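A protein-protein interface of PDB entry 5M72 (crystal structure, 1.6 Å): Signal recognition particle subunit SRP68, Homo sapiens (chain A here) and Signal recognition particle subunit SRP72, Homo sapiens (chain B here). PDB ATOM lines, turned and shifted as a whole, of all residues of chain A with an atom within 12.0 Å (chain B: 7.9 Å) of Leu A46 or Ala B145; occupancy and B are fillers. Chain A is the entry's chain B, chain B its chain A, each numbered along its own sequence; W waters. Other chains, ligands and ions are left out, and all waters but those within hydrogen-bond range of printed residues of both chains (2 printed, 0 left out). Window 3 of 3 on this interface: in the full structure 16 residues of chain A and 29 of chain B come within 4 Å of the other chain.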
ATOM      1  N   LYS A  44       1.766  12.635   7.314  1.00  0.00           N
ATOM      2  CA  LYS A  44       3.113  13.032   7.707  1.00  0.00           C
ATOM      3  C   LYS A  44       3.100  13.954   8.923  1.00  0.00           C
ATOM      4  O   LYS A  44       2.619  15.084   8.844  1.00  0.00           O
ATOM      5  CB  LYS A  44       3.827  13.723   6.542  1.00  0.00           C
ATOM      6  CG  LYS A  44       4.726  12.811   5.725  1.00  0.00           C
ATOM      7  CD  LYS A  44       5.251  13.521   4.484  1.00  0.00           C
ATOM      8  CE  LYS A  44       5.826  14.889   4.821  1.00  0.00           C
ATOM      9  NZ  LYS A  44       6.941  14.808   5.804  1.00  0.00           N
ATOM     10  N   PRO A  45       3.615  13.470  10.050  1.00  0.00           N
ATOM     11  CA  PRO A  45       3.791  14.349  11.210  1.00  0.00           C
ATOM     12  C   PRO A  45       4.842  15.411  10.932  1.00  0.00           C
ATOM     13  O   PRO A  45       5.659  15.299  10.015  1.00  0.00           O
ATOM     14  CB  PRO A  45       4.246  13.396  12.322  1.00  0.00           C
ATOM     15  CG  PRO A  45       3.827  12.034  11.864  1.00  0.00           C
ATOM     16  CD  PRO A  45       3.929  12.067  10.367  1.00  0.00           C
ATOM     17  N   LEU A  46       4.804  16.462  11.745  1.00  0.00           N
ATOM     18  CA  LEU A  46       5.786  17.532  11.638  1.00  0.00           C
ATOM     19  C   LEU A  46       7.167  17.006  12.011  1.00  0.00           C
ATOM     20  O   LEU A  46       7.334  16.357  13.049  1.00  0.00           O
ATOM     21  CB  LEU A  46       5.378  18.691  12.546  1.00  0.00           C
ATOM     22  CG  LEU A  46       6.281  19.912  12.676  1.00  0.00           C
ATOM     23  CD1 LEU A  46       6.429  20.618  11.340  1.00  0.00           C
ATOM     24  CD2 LEU A  46       5.706  20.848  13.727  1.00  0.00           C
ATOM     25  N   PHE A  47       8.158  17.275  11.156  1.00  0.00           N
ATOM     26  CA  PHE A  47       9.518  16.791  11.376  1.00  0.00           C
ATOM     27  C   PHE A  47      10.490  17.853  10.874  1.00  0.00           C
ATOM     28  O   PHE A  47      10.398  18.287   9.718  1.00  0.00           O
ATOM     29  CB  PHE A  47       9.738  15.441  10.669  1.00  0.00           C
ATOM     30  CG  PHE A  47      10.946  14.684  11.159  1.00  0.00           C
ATOM     31  CD1 PHE A  47      12.166  14.799  10.507  1.00  0.00           C
ATOM     32  CD2 PHE A  47      10.865  13.870  12.279  1.00  0.00           C
ATOM     33  CE1 PHE A  47      13.280  14.109  10.958  1.00  0.00           C
ATOM     34  CE2 PHE A  47      11.980  13.181  12.740  1.00  0.00           C
ATOM     35  CZ  PHE A  47      13.186  13.297  12.081  1.00  0.00           C
ATOM     36  N   PHE A  48      11.415  18.278  11.736  1.00  0.00           N
ATOM     37  CA  PHE A  48      12.302  19.407  11.463  1.00  0.00           C
ATOM     38  C   PHE A  48      13.681  18.942  11.009  1.00  0.00           C
ATOM     39  O   PHE A  48      14.274  18.041  11.604  1.00  0.00           O
ATOM     40  CB  PHE A  48      12.463  20.282  12.709  1.00  0.00           C
ATOM     41  CG  PHE A  48      11.203  20.979  13.131  1.00  0.00           C
ATOM     42  CD1 PHE A  48      10.355  20.407  14.065  1.00  0.00           C
ATOM     43  CD2 PHE A  48      10.878  22.217  12.602  1.00  0.00           C
ATOM     44  CE1 PHE A  48       9.196  21.057  14.458  1.00  0.00           C
ATOM     45  CE2 PHE A  48       9.726  22.874  12.983  1.00  0.00           C
ATOM     46  CZ  PHE A  48       8.881  22.295  13.916  1.00  0.00           C
ATOM     47  N   ASP A  49      14.216  19.598   9.977  1.00  0.00           N
ATOM     48  CA  ASP A  49      15.591  19.351   9.537  1.00  0.00           C
ATOM     49  C   ASP A  49      16.530  20.154  10.433  1.00  0.00           C
ATOM     50  O   ASP A  49      17.006  21.238  10.081  1.00  0.00           O
ATOM     51  CB  ASP A  49      15.756  19.727   8.068  1.00  0.00           C
ATOM     52  CG  ASP A  49      17.190  19.567   7.561  1.00  0.00           C
ATOM     53  OD1 ASP A  49      18.044  19.032   8.294  1.00  0.00           O
ATOM     54  OD2 ASP A  49      17.462  19.974   6.406  1.00  0.00           O
ATOM     55  N   LEU A  50      16.809  19.603  11.617  1.00  0.00           N
ATOM     56  CA  LEU A  50      17.710  20.288  12.539  1.00  0.00           C
ATOM     57  C   LEU A  50      19.164  20.204  12.090  1.00  0.00           C
ATOM     58  O   LEU A  50      19.974  21.054  12.495  1.00  0.00           O
ATOM     59  CB  LEU A  50      17.550  19.719  13.948  1.00  0.00           C
ATOM     60  CG  LEU A  50      16.160  19.956  14.545  1.00  0.00           C
ATOM     61  CD1 LEU A  50      16.073  19.389  15.948  1.00  0.00           C
ATOM     62  CD2 LEU A  50      15.803  21.435  14.550  1.00  0.00           C
ATOM     63  N   TYR B 112      15.143   8.075  10.348  1.00  0.00           N
ATOM     64  CA  TYR B 112      13.710   8.333  10.240  1.00  0.00           C
ATOM     65  C   TYR B 112      13.233   8.145   8.804  1.00  0.00           C
ATOM     66  O   TYR B 112      12.239   7.454   8.543  1.00  0.00           O
ATOM     67  CB  TYR B 112      13.402   9.749  10.746  1.00  0.00           C
ATOM     68  CG  TYR B 112      11.935  10.105  10.727  1.00  0.00           C
ATOM     69  CD1 TYR B 112      11.052   9.547  11.650  1.00  0.00           C
ATOM     70  CD2 TYR B 112      11.431  11.002   9.797  1.00  0.00           C
ATOM     71  CE1 TYR B 112       9.709   9.871  11.639  1.00  0.00           C
ATOM     72  CE2 TYR B 112      10.086  11.331   9.777  1.00  0.00           C
ATOM     73  CZ  TYR B 112       9.231  10.765  10.704  1.00  0.00           C
ATOM     74  OH  TYR B 112       7.895  11.088  10.694  1.00  0.00           O
ATOM     75  N   TYR B 117      12.793   2.879  12.865  1.00  0.00           N
ATOM     76  CA  TYR B 117      12.264   3.712  13.944  1.00  0.00           C
ATOM     77  C   TYR B 117      12.833   3.334  15.310  1.00  0.00           C
ATOM     78  O   TYR B 117      13.000   4.205  16.169  1.00  0.00           O
ATOM     79  CB  TYR B 117      10.739   3.640  13.962  1.00  0.00           C
ATOM     80  CG  TYR B 117      10.097   4.146  12.690  1.00  0.00           C
ATOM     81  CD1 TYR B 117      10.421   5.395  12.171  1.00  0.00           C
ATOM     82  CD2 TYR B 117       9.178   3.374  11.999  1.00  0.00           C
ATOM     83  CE1 TYR B 117       9.836   5.862  11.005  1.00  0.00           C
ATOM     84  CE2 TYR B 117       8.592   3.829  10.829  1.00  0.00           C
ATOM     85  CZ  TYR B 117       8.923   5.069  10.340  1.00  0.00           C
ATOM     86  OH  TYR B 117       8.335   5.516   9.182  1.00  0.00           O
ATOM     87  N   CYS B 120      16.164   4.824  15.385  1.00  0.00           N
ATOM     88  CA  CYS B 120      15.940   6.264  15.357  1.00  0.00           C
ATOM     89  C   CYS B 120      15.529   6.783  16.730  1.00  0.00           C
ATOM     90  O   CYS B 120      16.017   7.824  17.187  1.00  0.00           O
ATOM     91  CB  CYS B 120      14.879   6.587  14.301  1.00  0.00           C
ATOM     92  SG  CYS B 120      14.539   8.334  14.055  1.00  0.00           S
ATOM     93  N   LEU B 121      14.653   6.053  17.424  1.00  0.00           N
ATOM     94  CA  LEU B 121      14.224   6.498  18.743  1.00  0.00           C
ATOM     95  C   LEU B 121      15.390   6.551  19.721  1.00  0.00           C
ATOM     96  O   LEU B 121      15.507   7.501  20.502  1.00  0.00           O
ATOM     97  CB  LEU B 121      13.121   5.576  19.269  1.00  0.00           C
ATOM     98  CG  LEU B 121      12.609   5.883  20.680  1.00  0.00           C
ATOM     99  CD1 LEU B 121      12.110   7.322  20.792  1.00  0.00           C
ATOM    100  CD2 LEU B 121      11.519   4.889  21.071  1.00  0.00           C
ATOM    101  N   GLU B 137      12.584  22.287  21.562  1.00  0.00           N
ATOM    102  CA  GLU B 137      11.178  22.070  21.220  1.00  0.00           C
ATOM    103  C   GLU B 137      11.046  21.334  19.898  1.00  0.00           C
ATOM    104  O   GLU B 137      10.250  20.393  19.765  1.00  0.00           O
ATOM    105  CB  GLU B 137      10.442  23.408  21.148  1.00  0.00           C
ATOM    106  CG  GLU B 137       9.984  23.944  22.485  1.00  0.00           C
ATOM    107  CD  GLU B 137       8.788  23.188  23.022  1.00  0.00           C
ATOM    108  OE1 GLU B 137       7.647  23.471  22.575  1.00  0.00           O
ATOM    109  OE2 GLU B 137       8.986  22.301  23.881  1.00  0.00           O
ATOM    110  N   GLU B 138      11.819  21.764  18.900  1.00  0.00           N
ATOM    111  CA  GLU B 138      11.789  21.107  17.602  1.00  0.00           C
ATOM    112  C   GLU B 138      12.278  19.673  17.709  1.00  0.00           C
ATOM    113  O   GLU B 138      11.695  18.761  17.107  1.00  0.00           O
ATOM    114  CB  GLU B 138      12.644  21.886  16.601  1.00  0.00           C
ATOM    115  CG  GLU B 138      12.072  23.229  16.201  1.00  0.00           C
ATOM    116  CD  GLU B 138      12.602  24.379  17.039  1.00  0.00           C
ATOM    117  OE1 GLU B 138      12.971  24.168  18.215  1.00  0.00           O
ATOM    118  OE2 GLU B 138      12.654  25.504  16.507  1.00  0.00           O
ATOM    119  N   ARG B 139      13.357  19.456  18.467  1.00  0.00           N
ATOM    120  CA  ARG B 139      13.916  18.113  18.564  1.00  0.00           C
ATOM    121  C   ARG B 139      12.968  17.172  19.291  1.00  0.00           C
ATOM    122  O   ARG B 139      12.905  15.986  18.960  1.00  0.00           O
ATOM    123  CB  ARG B 139      15.280  18.154  19.258  1.00  0.00           C
ATOM    124  CG  ARG B 139      16.108  16.883  19.064  1.00  0.00           C
ATOM    125  CD  ARG B 139      17.533  17.046  19.588  1.00  0.00           C
ATOM    126  NE  ARG B 139      18.330  17.918  18.725  1.00  0.00           N
ATOM    127  CZ  ARG B 139      18.642  19.182  18.995  1.00  0.00           C
ATOM    128  NH1 ARG B 139      18.249  19.755  20.128  1.00  0.00           N
ATOM    129  NH2 ARG B 139      19.364  19.877  18.128  1.00  0.00           N
ATOM    130  N   LYS B 140      12.215  17.682  20.265  1.00  0.00           N
ATOM    131  CA  LYS B 140      11.234  16.844  20.939  1.00  0.00           C
ATOM    132  C   LYS B 140      10.035  16.563  20.044  1.00  0.00           C
ATOM    133  O   LYS B 140       9.413  15.499  20.160  1.00  0.00           O
ATOM    134  CB  LYS B 140      10.815  17.501  22.255  1.00  0.00           C
ATOM    135  CG  LYS B 140      11.919  17.464  23.310  1.00  0.00           C
ATOM    136  CD  LYS B 140      11.499  18.153  24.592  1.00  0.00           C
ATOM    137  CE  LYS B 140      12.543  17.972  25.680  1.00  0.00           C
ATOM    138  NZ  LYS B 140      12.225  18.792  26.883  1.00  0.00           N
ATOM    139  N   THR B 141       9.706  17.490  19.140  1.00  0.00           N
ATOM    140  CA  THR B 141       8.708  17.208  18.113  1.00  0.00           C
ATOM    141  C   THR B 141       9.171  16.071  17.209  1.00  0.00           C
ATOM    142  O   THR B 141       8.390  15.173  16.877  1.00  0.00           O
ATOM    143  CB  THR B 141       8.422  18.472  17.293  1.00  0.00           C
ATOM    144  OG1 THR B 141       7.817  19.466  18.130  1.00  0.00           O
ATOM    145  CG2 THR B 141       7.478  18.165  16.129  1.00  0.00           C
ATOM    146  N   ASN B 142      10.443  16.099  16.796  1.00  0.00           N
ATOM    147  CA  ASN B 142      11.004  15.002  16.011  1.00  0.00           C
ATOM    148  C   ASN B 142      10.915  13.684  16.766  1.00  0.00           C
ATOM    149  O   ASN B 142      10.517  12.655  16.203  1.00  0.00           O
ATOM    150  CB  ASN B 142      12.458  15.309  15.648  1.00  0.00           C
ATOM    151  CG  ASN B 142      12.577  16.287  14.504  1.00  0.00           C
ATOM    152  OD1 ASN B 142      11.622  16.970  14.148  1.00  0.00           O
ATOM    153  ND2 ASN B 142      13.759  16.348  13.916  1.00  0.00           N
ATOM    154  N   LEU B 143      11.297  13.697  18.042  1.00  0.00           N
ATOM    155  CA  LEU B 143      11.202  12.484  18.848  1.00  0.00           C
ATOM    156  C   LEU B 143       9.767  11.965  18.893  1.00  0.00           C
ATOM    157  O   LEU B 143       9.537  10.755  18.771  1.00  0.00           O
ATOM    158  CB  LEU B 143      11.751  12.751  20.256  1.00  0.00           C
ATOM    159  CG  LEU B 143      11.824  11.563  21.238  1.00  0.00           C
ATOM    160  CD1 LEU B 143      13.021  11.704  22.176  1.00  0.00           C
ATOM    161  CD2 LEU B 143      10.553  11.453  22.050  1.00  0.00           C
ATOM    162  N   SER B 144       8.787  12.863  19.033  1.00  0.00           N
ATOM    163  CA  SER B 144       7.391  12.432  19.075  1.00  0.00           C
ATOM    164  C   SER B 144       6.936  11.834  17.751  1.00  0.00           C
ATOM    165  O   SER B 144       6.096  10.925  17.740  1.00  0.00           O
ATOM    166  CB  SER B 144       6.482  13.599  19.451  1.00  0.00           C
ATOM    167  OG  SER B 144       6.713  14.006  20.784  1.00  0.00           O
ATOM    168  N   ALA B 145       7.449  12.345  16.629  1.00  0.00           N
ATOM    169  CA  ALA B 145       7.131  11.752  15.334  1.00  0.00           C
ATOM    170  C   ALA B 145       7.649  10.321  15.245  1.00  0.00           C
ATOM    171  O   ALA B 145       7.000   9.451  14.647  1.00  0.00           O
ATOM    172  CB  ALA B 145       7.707  12.613  14.206  1.00  0.00           C
ATOM    173  N   VAL B 146       8.817  10.056  15.837  1.00  0.00           N
ATOM    174  CA  VAL B 146       9.357   8.697  15.843  1.00  0.00           C
ATOM    175  C   VAL B 146       8.486   7.782  16.695  1.00  0.00           C
ATOM    176  O   VAL B 146       8.151   6.662  16.284  1.00  0.00           O
ATOM    177  CB  VAL B 146      10.818   8.701  16.324  1.00  0.00           C
ATOM    178  CG1 VAL B 146      11.427   7.309  16.197  1.00  0.00           C
ATOM    179  CG2 VAL B 146      11.633   9.709  15.530  1.00  0.00           C
ATOM    180  N   VAL B 147       8.097   8.247  17.891  1.00  0.00           N
ATOM    181  CA  VAL B 147       7.226   7.450  18.761  1.00  0.00           C
ATOM    182  C   VAL B 147       5.906   7.150  18.065  1.00  0.00           C
ATOM    183  O   VAL B 147       5.368   6.040  18.175  1.00  0.00           O
ATOM    184  CB  VAL B 147       7.004   8.171  20.105  1.00  0.00           C
ATOM    185  CG1 VAL B 147       5.989   7.392  20.987  1.00  0.00           C
ATOM    186  CG2 VAL B 147       8.311   8.310  20.860  1.00  0.00           C
ATOM    187  N   ALA B 148       5.359   8.132  17.346  1.00  0.00           N
ATOM    188  CA  ALA B 148       4.101   7.913  16.636  1.00  0.00           C
ATOM    189  C   ALA B 148       4.256   6.876  15.531  1.00  0.00           C
ATOM    190  O   ALA B 148       3.369   6.036  15.328  1.00  0.00           O
ATOM    191  CB  ALA B 148       3.586   9.232  16.065  1.00  0.00           C
ATOM    192  N   ALA B 149       5.377   6.916  14.806  1.00  0.00           N
ATOM    193  CA  ALA B 149       5.585   5.962  13.723  1.00  0.00           C
ATOM    194  C   ALA B 149       5.672   4.537  14.248  1.00  0.00           C
ATOM    195  O   ALA B 149       5.266   3.592  13.558  1.00  0.00           O
ATOM    196  CB  ALA B 149       6.847   6.323  12.941  1.00  0.00           C
ATOM    197  N   GLN B 150       6.186   4.360  15.466  1.00  0.00           N
ATOM    198  CA  GLN B 150       6.254   3.023  16.044  1.00  0.00           C
ATOM    199  C   GLN B 150       4.872   2.475  16.378  1.00  0.00           C
ATOM    200  O   GLN B 150       4.687   1.255  16.418  1.00  0.00           O
ATOM    201  CB  GLN B 150       7.123   3.037  17.297  1.00  0.00           C
ATOM    202  CG  GLN B 150       8.605   3.120  17.026  1.00  0.00           C
ATOM    203  CD  GLN B 150       9.395   3.212  18.308  1.00  0.00           C
ATOM    204  OE1 GLN B 150       9.026   3.953  19.218  1.00  0.00           O
ATOM    205  NE2 GLN B 150      10.476   2.446  18.398  1.00  0.00           N
ATOM    206  N   SER B 151       3.899   3.345  16.627  1.00  0.00           N
ATOM    207  CA  SER B 151       2.563   2.889  17.003  1.00  0.00           C
ATOM    208  C   SER B 151       1.588   2.977  15.833  1.00  0.00           C
ATOM    209  O   SER B 151       1.981   2.852  14.673  1.00  0.00           O
ATOM    210  CB  SER B 151       2.037   3.702  18.184  1.00  0.00           C
ATOM    211  OG  SER B 151       1.880   5.066  17.832  1.00  0.00           O
HETATM  212  O   HOH W   1       5.894  15.331  15.233  1.00  0.00           O
HETATM  213  O   HOH W   2       6.874  12.913   9.129  1.00  0.00           O
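N of Phe A48 is in hydrogen-bond range of OD1 of Asn B142, at 2.8 Å.
SG of Cys B120 lies within hydrogen-bond range of N of Tyr B112 (3.8 Å).
O of Glu B138 sits close to OD1 of Asn B142 (3.5 Å).
The backbone carbonyl oxygen (O) of Glu B137 sits at hydrogen-bond distance from the side-chain hydroxyl (OG1) of Thr B141 (3.1 Å).
CG2 of Thr B141 touches O of Leu A46 (3.6 Å).
O of Leu A46 touches CB of Ala B145 (3.9 Å).
Tyr B112 touches Phe A47.
Phe A47 touches Asn B142 (CA to OD1, 3.5 Å).
Ala B145 touches Phe A47.
CD1 of Phe A48 touches O of Glu B138 (3.7 Å).
Phe A48 touches Thr B141.
Glu B138 touches Leu A50.
Arg B139 touches Leu A50 (CB to CD1, 3.6 Å).
Pro A45 touches none of the printed residues of chain B.
Of chain B, only Thr B141 and Ala B145 come within 4 Å of Leu A46.
Printed residues of chain B within 4 Å of Phe A48: Glu B138 (3.7 Å), Thr B141 (3.8 Å) and Asn B142 (2.8 Å).
Printed residues of chain B within 4 Å of Leu A50: Glu B138 and Arg B139.
Of the printed residues of chain A, Tyr B112 touches Phe A47.
Printed residues of chain A within 4 Å of Arg B139: Leu A50.
Of chain A, only Leu A46 (3.6 Å) and Phe A48 (3.8 Å) come within 4 Å of Thr B141.
No residue of chain A comes within 4 Å of Leu B143.
No residue of chain A comes within 4 Å of Ser B144.
No residue of chain A comes within 4 Å of Val B146.
No residue of chain A comes within 4 Å of Val B147.
The nearest residue of chain B that does not touch Leu A46 is Asn B142 (4.5 Å).
Of the 19 printed residues of chain B, 6 touch a printed residue of chain A.
Printed residues of chain A that touch a printed residue of chain B: Leu A46, Phe A47, Phe A48 and Leu A50.
Among the printed residues, no Asp or Glu carboxylate lies within 4 Å of a Lys or Arg side-chain nitrogen of the other chain.
Water W2 bridges the side-chain hydroxyl of Tyr B112 (2.6 Å) and the backbone carbonyl oxygen of Pro A45 (2.8 Å).
Water W1 lies within hydrogen-bond range of O of Leu A46 (2.8 Å) and O of Thr B141 (3.0 Å).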
